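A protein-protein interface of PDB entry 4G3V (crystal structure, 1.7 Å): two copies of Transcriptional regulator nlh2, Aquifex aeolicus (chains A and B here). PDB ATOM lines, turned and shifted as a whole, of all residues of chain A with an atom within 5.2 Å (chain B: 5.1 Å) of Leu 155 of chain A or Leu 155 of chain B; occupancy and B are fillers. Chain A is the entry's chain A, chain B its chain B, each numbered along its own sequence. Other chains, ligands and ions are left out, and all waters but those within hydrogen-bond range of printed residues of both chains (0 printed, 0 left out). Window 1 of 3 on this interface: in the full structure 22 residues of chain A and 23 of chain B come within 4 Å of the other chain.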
ATOM      1  N   VAL A  12      -8.681   8.283  20.873  1.00  0.00           N
ATOM      2  CA  VAL A  12      -9.853   8.895  20.259  1.00  0.00           C
ATOM      3  C   VAL A  12      -9.428   9.737  19.045  1.00  0.00           C
ATOM      4  O   VAL A  12     -10.042   9.653  17.972  1.00  0.00           O
ATOM      5  CB  VAL A  12     -10.640   9.743  21.284  1.00  0.00           C
ATOM      6  CG1 VAL A  12     -11.588  10.718  20.582  1.00  0.00           C
ATOM      7  CG2 VAL A  12     -11.398   8.822  22.236  1.00  0.00           C
ATOM      8  N   ILE A  15      -8.422   7.174  16.287  1.00  0.00           N
ATOM      9  CA  ILE A  15      -9.590   6.519  15.719  1.00  0.00           C
ATOM     10  C   ILE A  15     -10.323   7.450  14.762  1.00  0.00           C
ATOM     11  O   ILE A  15     -10.748   7.025  13.693  1.00  0.00           O
ATOM     12  CB  ILE A  15     -10.519   5.976  16.840  1.00  0.00           C
ATOM     13  CG1 ILE A  15      -9.846   4.752  17.495  1.00  0.00           C
ATOM     14  CG2 ILE A  15     -11.878   5.589  16.287  1.00  0.00           C
ATOM     15  CD1 ILE A  15     -10.523   4.258  18.779  1.00  0.00           C
ATOM     16  N   THR A  16     -10.440   8.732  15.114  1.00  0.00           N
ATOM     17  CA  THR A  16     -11.115   9.680  14.228  1.00  0.00           C
ATOM     18  C   THR A  16     -10.342   9.839  12.920  1.00  0.00           C
ATOM     19  O   THR A  16     -10.929   9.925  11.841  1.00  0.00           O
ATOM     20  CB  THR A  16     -11.297  11.040  14.933  1.00  0.00           C
ATOM     21  OG1 THR A  16     -12.079  10.843  16.116  1.00  0.00           O
ATOM     22  CG2 THR A  16     -11.990  12.060  14.061  1.00  0.00           C
ATOM     23  N   LEU A  19     -11.053   6.695  10.840  1.00  0.00           N
ATOM     24  CA  LEU A  19     -12.420   6.644  10.349  1.00  0.00           C
ATOM     25  C   LEU A  19     -12.792   7.772   9.375  1.00  0.00           C
ATOM     26  O   LEU A  19     -13.816   7.688   8.693  1.00  0.00           O
ATOM     27  CB  LEU A  19     -13.392   6.620  11.524  1.00  0.00           C
ATOM     28  CG  LEU A  19     -13.255   5.409  12.452  1.00  0.00           C
ATOM     29  CD1 LEU A  19     -14.272   5.514  13.582  1.00  0.00           C
ATOM     30  CD2 LEU A  19     -13.426   4.099  11.684  1.00  0.00           C
ATOM     31  N   VAL A 151     -17.562   6.553  23.906  1.00  0.00           N
ATOM     32  CA  VAL A 151     -17.143   7.534  22.912  1.00  0.00           C
ATOM     33  C   VAL A 151     -16.805   6.830  21.604  1.00  0.00           C
ATOM     34  O   VAL A 151     -17.200   7.277  20.532  1.00  0.00           O
ATOM     35  CB  VAL A 151     -15.924   8.338  23.381  1.00  0.00           C
ATOM     36  CG1 VAL A 151     -15.286   9.074  22.206  1.00  0.00           C
ATOM     37  CG2 VAL A 151     -16.326   9.318  24.481  1.00  0.00           C
ATOM     38  N   ILE A 152     -16.107   5.700  21.694  1.00  0.00           N
ATOM     39  CA  ILE A 152     -15.722   4.980  20.483  1.00  0.00           C
ATOM     40  C   ILE A 152     -16.958   4.445  19.749  1.00  0.00           C
ATOM     41  O   ILE A 152     -17.024   4.489  18.528  1.00  0.00           O
ATOM     42  CB  ILE A 152     -14.698   3.897  20.794  1.00  0.00           C
ATOM     43  CG1 ILE A 152     -13.386   4.592  21.215  1.00  0.00           C
ATOM     44  CG2 ILE A 152     -14.462   2.994  19.566  1.00  0.00           C
ATOM     45  CD1 ILE A 152     -12.372   3.690  21.761  1.00  0.00           C
ATOM     46  N   GLY A 153     -17.970   4.008  20.489  1.00  0.00           N
ATOM     47  CA  GLY A 153     -19.213   3.581  19.868  1.00  0.00           C
ATOM     48  C   GLY A 153     -19.872   4.707  19.083  1.00  0.00           C
ATOM     49  O   GLY A 153     -20.424   4.500  17.999  1.00  0.00           O
ATOM     50  N   ASN A 154     -19.800   5.915  19.622  1.00  0.00           N
ATOM     51  CA  ASN A 154     -20.316   7.089  18.930  1.00  0.00           C
ATOM     52  C   ASN A 154     -19.519   7.456  17.665  1.00  0.00           C
ATOM     53  O   ASN A 154     -20.104   7.802  16.626  1.00  0.00           O
ATOM     54  CB  ASN A 154     -20.368   8.265  19.885  1.00  0.00           C
ATOM     55  CG  ASN A 154     -21.588   8.199  20.807  1.00  0.00           C
ATOM     56  OD1 ASN A 154     -22.686   8.522  20.396  1.00  0.00           O
ATOM     57  ND2 ASN A 154     -21.393   7.760  22.035  1.00  0.00           N
ATOM     58  N   LEU A 155     -18.192   7.384  17.751  1.00  0.00           N
ATOM     59  CA  LEU A 155     -17.361   7.603  16.575  1.00  0.00           C
ATOM     60  C   LEU A 155     -17.732   6.586  15.517  1.00  0.00           C
ATOM     61  O   LEU A 155     -17.791   6.898  14.319  1.00  0.00           O
ATOM     62  CB  LEU A 155     -15.883   7.487  16.920  1.00  0.00           C
ATOM     63  CG  LEU A 155     -15.313   8.543  17.862  1.00  0.00           C
ATOM     64  CD1 LEU A 155     -13.874   8.208  18.196  1.00  0.00           C
ATOM     65  CD2 LEU A 155     -15.408   9.928  17.265  1.00  0.00           C
ATOM     66  N   LEU A 156     -17.972   5.355  15.943  1.00  0.00           N
ATOM     67  CA  LEU A 156     -18.357   4.323  14.992  1.00  0.00           C
ATOM     68  C   LEU A 156     -19.751   4.608  14.390  1.00  0.00           C
ATOM     69  O   LEU A 156     -20.005   4.314  13.222  1.00  0.00           O
ATOM     70  CB  LEU A 156     -18.312   2.943  15.660  1.00  0.00           C
ATOM     71  CG  LEU A 156     -16.891   2.417  15.892  1.00  0.00           C
ATOM     72  CD1 LEU A 156     -16.872   1.226  16.843  1.00  0.00           C
ATOM     73  CD2 LEU A 156     -16.231   2.015  14.544  1.00  0.00           C
ATOM     74  N   GLY A 157     -20.655   5.169  15.188  1.00  0.00           N
ATOM     75  CA  GLY A 157     -21.964   5.558  14.678  1.00  0.00           C
ATOM     76  C   GLY A 157     -21.818   6.554  13.533  1.00  0.00           C
ATOM     77  O   GLY A 157     -22.465   6.444  12.503  1.00  0.00           O
ATOM     78  N   MET A 158     -20.942   7.540  13.707  1.00  0.00           N
ATOM     79  CA  MET A 158     -20.665   8.525  12.665  1.00  0.00           C
ATOM     80  C   MET A 158     -20.130   7.811  11.427  1.00  0.00           C
ATOM     81  O   MET A 158     -20.520   8.108  10.305  1.00  0.00           O
ATOM     82  CB  MET A 158     -19.631   9.551  13.133  1.00  0.00           C
ATOM     83  CG  MET A 158     -20.060  10.445  14.294  1.00  0.00           C
ATOM     84  SD  MET A 158     -21.341  11.634  13.889  1.00  0.00           S
ATOM     85  CE  MET A 158     -20.602  12.545  12.542  1.00  0.00           C
ATOM     86  N   PHE A 159     -19.228   6.860  11.657  1.00  0.00           N
ATOM     87  CA  PHE A 159     -18.611   6.110  10.563  1.00  0.00           C
ATOM     88  C   PHE A 159     -19.655   5.302   9.784  1.00  0.00           C
ATOM     89  O   PHE A 159     -19.611   5.245   8.546  1.00  0.00           O
ATOM     90  CB  PHE A 159     -17.542   5.169  11.094  1.00  0.00           C
ATOM     91  CG  PHE A 159     -16.745   4.473  10.012  1.00  0.00           C
ATOM     92  CD1 PHE A 159     -15.927   5.193   9.170  1.00  0.00           C
ATOM     93  CD2 PHE A 159     -16.823   3.098   9.849  1.00  0.00           C
ATOM     94  CE1 PHE A 159     -15.191   4.552   8.178  1.00  0.00           C
ATOM     95  CE2 PHE A 159     -16.095   2.450   8.877  1.00  0.00           C
ATOM     96  CZ  PHE A 159     -15.275   3.176   8.036  1.00  0.00           C
ATOM     97  N   VAL B  12     -22.668  13.716  24.542  1.00  0.00           N
ATOM     98  CA  VAL B  12     -21.963  13.066  23.433  1.00  0.00           C
ATOM     99  C   VAL B  12     -22.928  12.196  22.626  1.00  0.00           C
ATOM    100  O   VAL B  12     -22.943  12.244  21.405  1.00  0.00           O
ATOM    101  CB  VAL B  12     -20.771  12.233  23.929  1.00  0.00           C
ATOM    102  CG1 VAL B  12     -20.254  11.309  22.822  1.00  0.00           C
ATOM    103  CG2 VAL B  12     -19.670  13.161  24.398  1.00  0.00           C
ATOM    104  N   ILE B  15     -25.195  14.528  20.627  1.00  0.00           N
ATOM    105  CA  ILE B  15     -24.503  15.195  19.522  1.00  0.00           C
ATOM    106  C   ILE B  15     -24.336  14.241  18.341  1.00  0.00           C
ATOM    107  O   ILE B  15     -24.509  14.623  17.169  1.00  0.00           O
ATOM    108  CB  ILE B  15     -23.166  15.773  20.001  1.00  0.00           C
ATOM    109  CG1 ILE B  15     -23.446  17.025  20.834  1.00  0.00           C
ATOM    110  CG2 ILE B  15     -22.251  16.109  18.818  1.00  0.00           C
ATOM    111  CD1 ILE B  15     -22.255  17.503  21.659  1.00  0.00           C
ATOM    112  N   THR B  16     -24.027  12.985  18.646  1.00  0.00           N
ATOM    113  CA  THR B  16     -23.925  11.983  17.602  1.00  0.00           C
ATOM    114  C   THR B  16     -25.262  11.801  16.879  1.00  0.00           C
ATOM    115  O   THR B  16     -25.309  11.670  15.659  1.00  0.00           O
ATOM    116  CB  THR B  16     -23.405  10.655  18.165  1.00  0.00           C
ATOM    117  OG1 THR B  16     -22.109  10.872  18.747  1.00  0.00           O
ATOM    118  CG2 THR B  16     -23.299   9.603  17.064  1.00  0.00           C
ATOM    119  N   LEU B  19     -25.683  14.864  14.548  1.00  0.00           N
ATOM    120  CA  LEU B  19     -24.743  14.874  13.424  1.00  0.00           C
ATOM    121  C   LEU B  19     -24.893  13.699  12.474  1.00  0.00           C
ATOM    122  O   LEU B  19     -24.337  13.725  11.363  1.00  0.00           O
ATOM    123  CB  LEU B  19     -23.314  14.954  13.938  1.00  0.00           C
ATOM    124  CG  LEU B  19     -22.982  16.197  14.766  1.00  0.00           C
ATOM    125  CD1 LEU B  19     -21.538  16.140  15.237  1.00  0.00           C
ATOM    126  CD2 LEU B  19     -23.244  17.476  13.978  1.00  0.00           C
ATOM    127  N   VAL B 151     -13.569  15.271  22.516  1.00  0.00           N
ATOM    128  CA  VAL B 151     -14.420  14.289  21.861  1.00  0.00           C
ATOM    129  C   VAL B 151     -15.369  14.983  20.889  1.00  0.00           C
ATOM    130  O   VAL B 151     -15.571  14.518  19.767  1.00  0.00           O
ATOM    131  CB  VAL B 151     -15.250  13.484  22.887  1.00  0.00           C
ATOM    132  CG1 VAL B 151     -16.341  12.716  22.205  1.00  0.00           C
ATOM    133  CG2 VAL B 151     -14.346  12.540  23.670  1.00  0.00           C
ATOM    134  N   ILE B 152     -15.943  16.107  21.310  1.00  0.00           N
ATOM    135  CA  ILE B 152     -16.899  16.798  20.457  1.00  0.00           C
ATOM    136  C   ILE B 152     -16.189  17.339  19.213  1.00  0.00           C
ATOM    137  O   ILE B 152     -16.726  17.285  18.103  1.00  0.00           O
ATOM    138  CB  ILE B 152     -17.633  17.912  21.230  1.00  0.00           C
ATOM    139  CG1 ILE B 152     -18.505  17.256  22.327  1.00  0.00           C
ATOM    140  CG2 ILE B 152     -18.484  18.743  20.273  1.00  0.00           C
ATOM    141  CD1 ILE B 152     -19.129  18.216  23.256  1.00  0.00           C
ATOM    142  N   GLY B 153     -14.958  17.817  19.375  1.00  0.00           N
ATOM    143  CA  GLY B 153     -14.173  18.239  18.217  1.00  0.00           C
ATOM    144  C   GLY B 153     -14.008  17.122  17.204  1.00  0.00           C
ATOM    145  O   GLY B 153     -14.082  17.332  15.971  1.00  0.00           O
ATOM    146  N   ASN B 154     -13.771  15.915  17.722  1.00  0.00           N
ATOM    147  CA  ASN B 154     -13.598  14.749  16.875  1.00  0.00           C
ATOM    148  C   ASN B 154     -14.894  14.346  16.180  1.00  0.00           C
ATOM    149  O   ASN B 154     -14.890  14.016  14.992  1.00  0.00           O
ATOM    150  CB  ASN B 154     -13.016  13.599  17.681  1.00  0.00           C
ATOM    151  CG  ASN B 154     -11.508  13.715  17.837  1.00  0.00           C
ATOM    152  OD1 ASN B 154     -10.762  13.512  16.881  1.00  0.00           O
ATOM    153  ND2 ASN B 154     -11.060  14.040  19.026  1.00  0.00           N
ATOM    154  N   LEU B 155     -16.009  14.391  16.896  1.00  0.00           N
ATOM    155  CA  LEU B 155     -17.298  14.116  16.261  1.00  0.00           C
ATOM    156  C   LEU B 155     -17.557  15.123  15.147  1.00  0.00           C
ATOM    157  O   LEU B 155     -18.088  14.770  14.098  1.00  0.00           O
ATOM    158  CB  LEU B 155     -18.433  14.170  17.294  1.00  0.00           C
ATOM    159  CG  LEU B 155     -18.416  13.052  18.356  1.00  0.00           C
ATOM    160  CD1 LEU B 155     -19.409  13.359  19.456  1.00  0.00           C
ATOM    161  CD2 LEU B 155     -18.736  11.697  17.748  1.00  0.00           C
ATOM    162  N   LEU B 156     -17.193  16.384  15.378  1.00  0.00           N
ATOM    163  CA  LEU B 156     -17.361  17.408  14.350  1.00  0.00           C
ATOM    164  C   LEU B 156     -16.447  17.126  13.134  1.00  0.00           C
ATOM    165  O   LEU B 156     -16.826  17.364  11.995  1.00  0.00           O
ATOM    166  CB  LEU B 156     -17.099  18.795  14.927  1.00  0.00           C
ATOM    167  CG  LEU B 156     -18.200  19.314  15.862  1.00  0.00           C
ATOM    168  CD1 LEU B 156     -17.729  20.575  16.619  1.00  0.00           C
ATOM    169  CD2 LEU B 156     -19.491  19.599  15.100  1.00  0.00           C
ATOM    170  N   GLY B 157     -15.243  16.629  13.382  1.00  0.00           N
ATOM    171  CA  GLY B 157     -14.366  16.217  12.293  1.00  0.00           C
ATOM    172  C   GLY B 157     -15.019  15.149  11.429  1.00  0.00           C
ATOM    173  O   GLY B 157     -14.997  15.219  10.201  1.00  0.00           O
ATOM    174  N   MET B 158     -15.642  14.165  12.059  1.00  0.00           N
ATOM    175  CA  MET B 158     -16.324  13.159  11.279  1.00  0.00           C
ATOM    176  C   MET B 158     -17.502  13.755  10.519  1.00  0.00           C
ATOM    177  O   MET B 158     -17.768  13.354   9.376  1.00  0.00           O
ATOM    178  CB  MET B 158     -16.736  12.009  12.167  1.00  0.00           C
ATOM    179  CG  MET B 158     -15.535  11.395  12.855  1.00  0.00           C
ATOM    180  SD  MET B 158     -15.947   9.855  13.615  1.00  0.00           S
ATOM    181  CE  MET B 158     -16.111   8.832  12.149  1.00  0.00           C
ATOM    182  N   PHE B 159     -18.176  14.735  11.115  1.00  0.00           N
ATOM    183  CA  PHE B 159     -19.293  15.401  10.440  1.00  0.00           C
ATOM    184  C   PHE B 159     -18.806  16.205   9.231  1.00  0.00           C
ATOM    185  O   PHE B 159     -19.456  16.223   8.181  1.00  0.00           O
ATOM    186  CB  PHE B 159     -20.020  16.305  11.424  1.00  0.00           C
ATOM    187  CG  PHE B 159     -21.267  16.947  10.864  1.00  0.00           C
ATOM    188  CD1 PHE B 159     -22.380  16.185  10.550  1.00  0.00           C
ATOM    189  CD2 PHE B 159     -21.327  18.321  10.674  1.00  0.00           C
ATOM    190  CE1 PHE B 159     -23.539  16.782  10.059  1.00  0.00           C
ATOM    191  CE2 PHE B 159     -22.476  18.927  10.184  1.00  0.00           C
ATOM    192  CZ  PHE B 159     -23.581  18.153   9.871  1.00  0.00           C
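OD1 of Asn 154 of chain B is in hydrogen-bond range of OG1 of Thr 16 of chain A (3.1 Å).
The side-chain amide oxygen (OD1) of Asn 154 of chain A lies within hydrogen-bond range of the side-chain hydroxyl (OG1) of Thr 16 of chain B, 2.9 Å away.
SD of Met 158 of chain B lies close to O of Leu 155 of chain A, at 3.6 Å.
OG1 of Thr 16 of chain A is in hydrogen-bond range of O of Val 12 of chain A (3.0 Å).
O of Val 12 of chain B lies within hydrogen-bond range of OG1 of Thr 16 of chain B.
Among the printed residues, pairs that only touch across the chains: Val 12 of chain A with Asn 154 of chain B, Thr 16 of chain A with Met 158 of chain B, Leu 19 of chain A with Met 158 of chain B, Val 151 of chain A with Val 151 of chain B, Asn 154 of chain A with Val 12 of chain B, Leu 155 of chain A with Leu 155 of chain B, Met 158 of chain A with Leu 19 of chain B, Met 158 of chain A with Leu 155 of chain B, Met 158 of chain A with Met 158 of chain B, Met 158 of chain A with Phe 159 of chain B and Phe 159 of chain A with Met 158 of chain B.
Printed residues of chain B within 4 Å of Leu 19 of chain A: Met 158 (3.6 Å).
Ile 152 of chain A touches none of the printed residues of chain B.
Of the printed residues of chain B, Leu 155 of chain A touches Leu 155 and Met 158.
Leu 156 of chain A touches none of the printed residues of chain B.
Of the printed residues of chain A, Leu 155 of chain B touches Leu 155 and Met 158.
Printed residues of chain A within 4 Å of Met 158 of chain B: Thr 16, Leu 19, Leu 155, Met 158 and Phe 159.
The nearest printed residue of chain A that does not touch Leu 155 of chain B is Asn 154 of chain A (4.3 Å).
The nearest printed residue of chain A that does not touch Leu 19 of chain B is Gly 157 of chain A (7.6 Å).
Of the 13 printed residues of chain B, 8 touch a printed residue of chain A.
Of the 13 printed residues of chain A, 8 touch a printed residue of chain B.
Printed residues of chain A that touch a printed residue of chain B: Val 12, Thr 16, Leu 19, Val 151, Asn 154, Leu 155, Met 158 and Phe 159.
Hydrophobic or aromatic side chains of chain A within 4 Å of the printed part of chain B: Val 12, Leu 19, Val 151, Leu 155 and Met 158.
Among the printed residues, 14 pairs touch across the chains.
Among the printed residues, no Asp or Glu carboxylate lies within 4 Å of a Lys or Arg side-chain nitrogen of the other chain.
Val 12 of chain A touches Asn 154 of chain B, and with the chains exchanged Asn 154 of chain A touches Val 12 of chain B.
Thr 16 of chain A touches Asn 154 of chain B, and with the chains exchanged Asn 154 of chain A touches Thr 16 of chain B.
Leu 19 of chain A touches Met 158 of chain B, and with the chains exchanged Met 158 of chain A touches Leu 19 of chain B.
Met 158 of chain A touches Phe 159 of chain B, and with the chains exchanged Phe 159 of chain A touches Met 158 of chain B.
Positions printed for both chains: 12, 15, 16, 19, 151, 152, 153, 154, 155, 156, 157, 158 and 159.
Of the 14 pairs that touch across the chains among the printed residues, 13 have their exchanged pair printed and touching as well.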
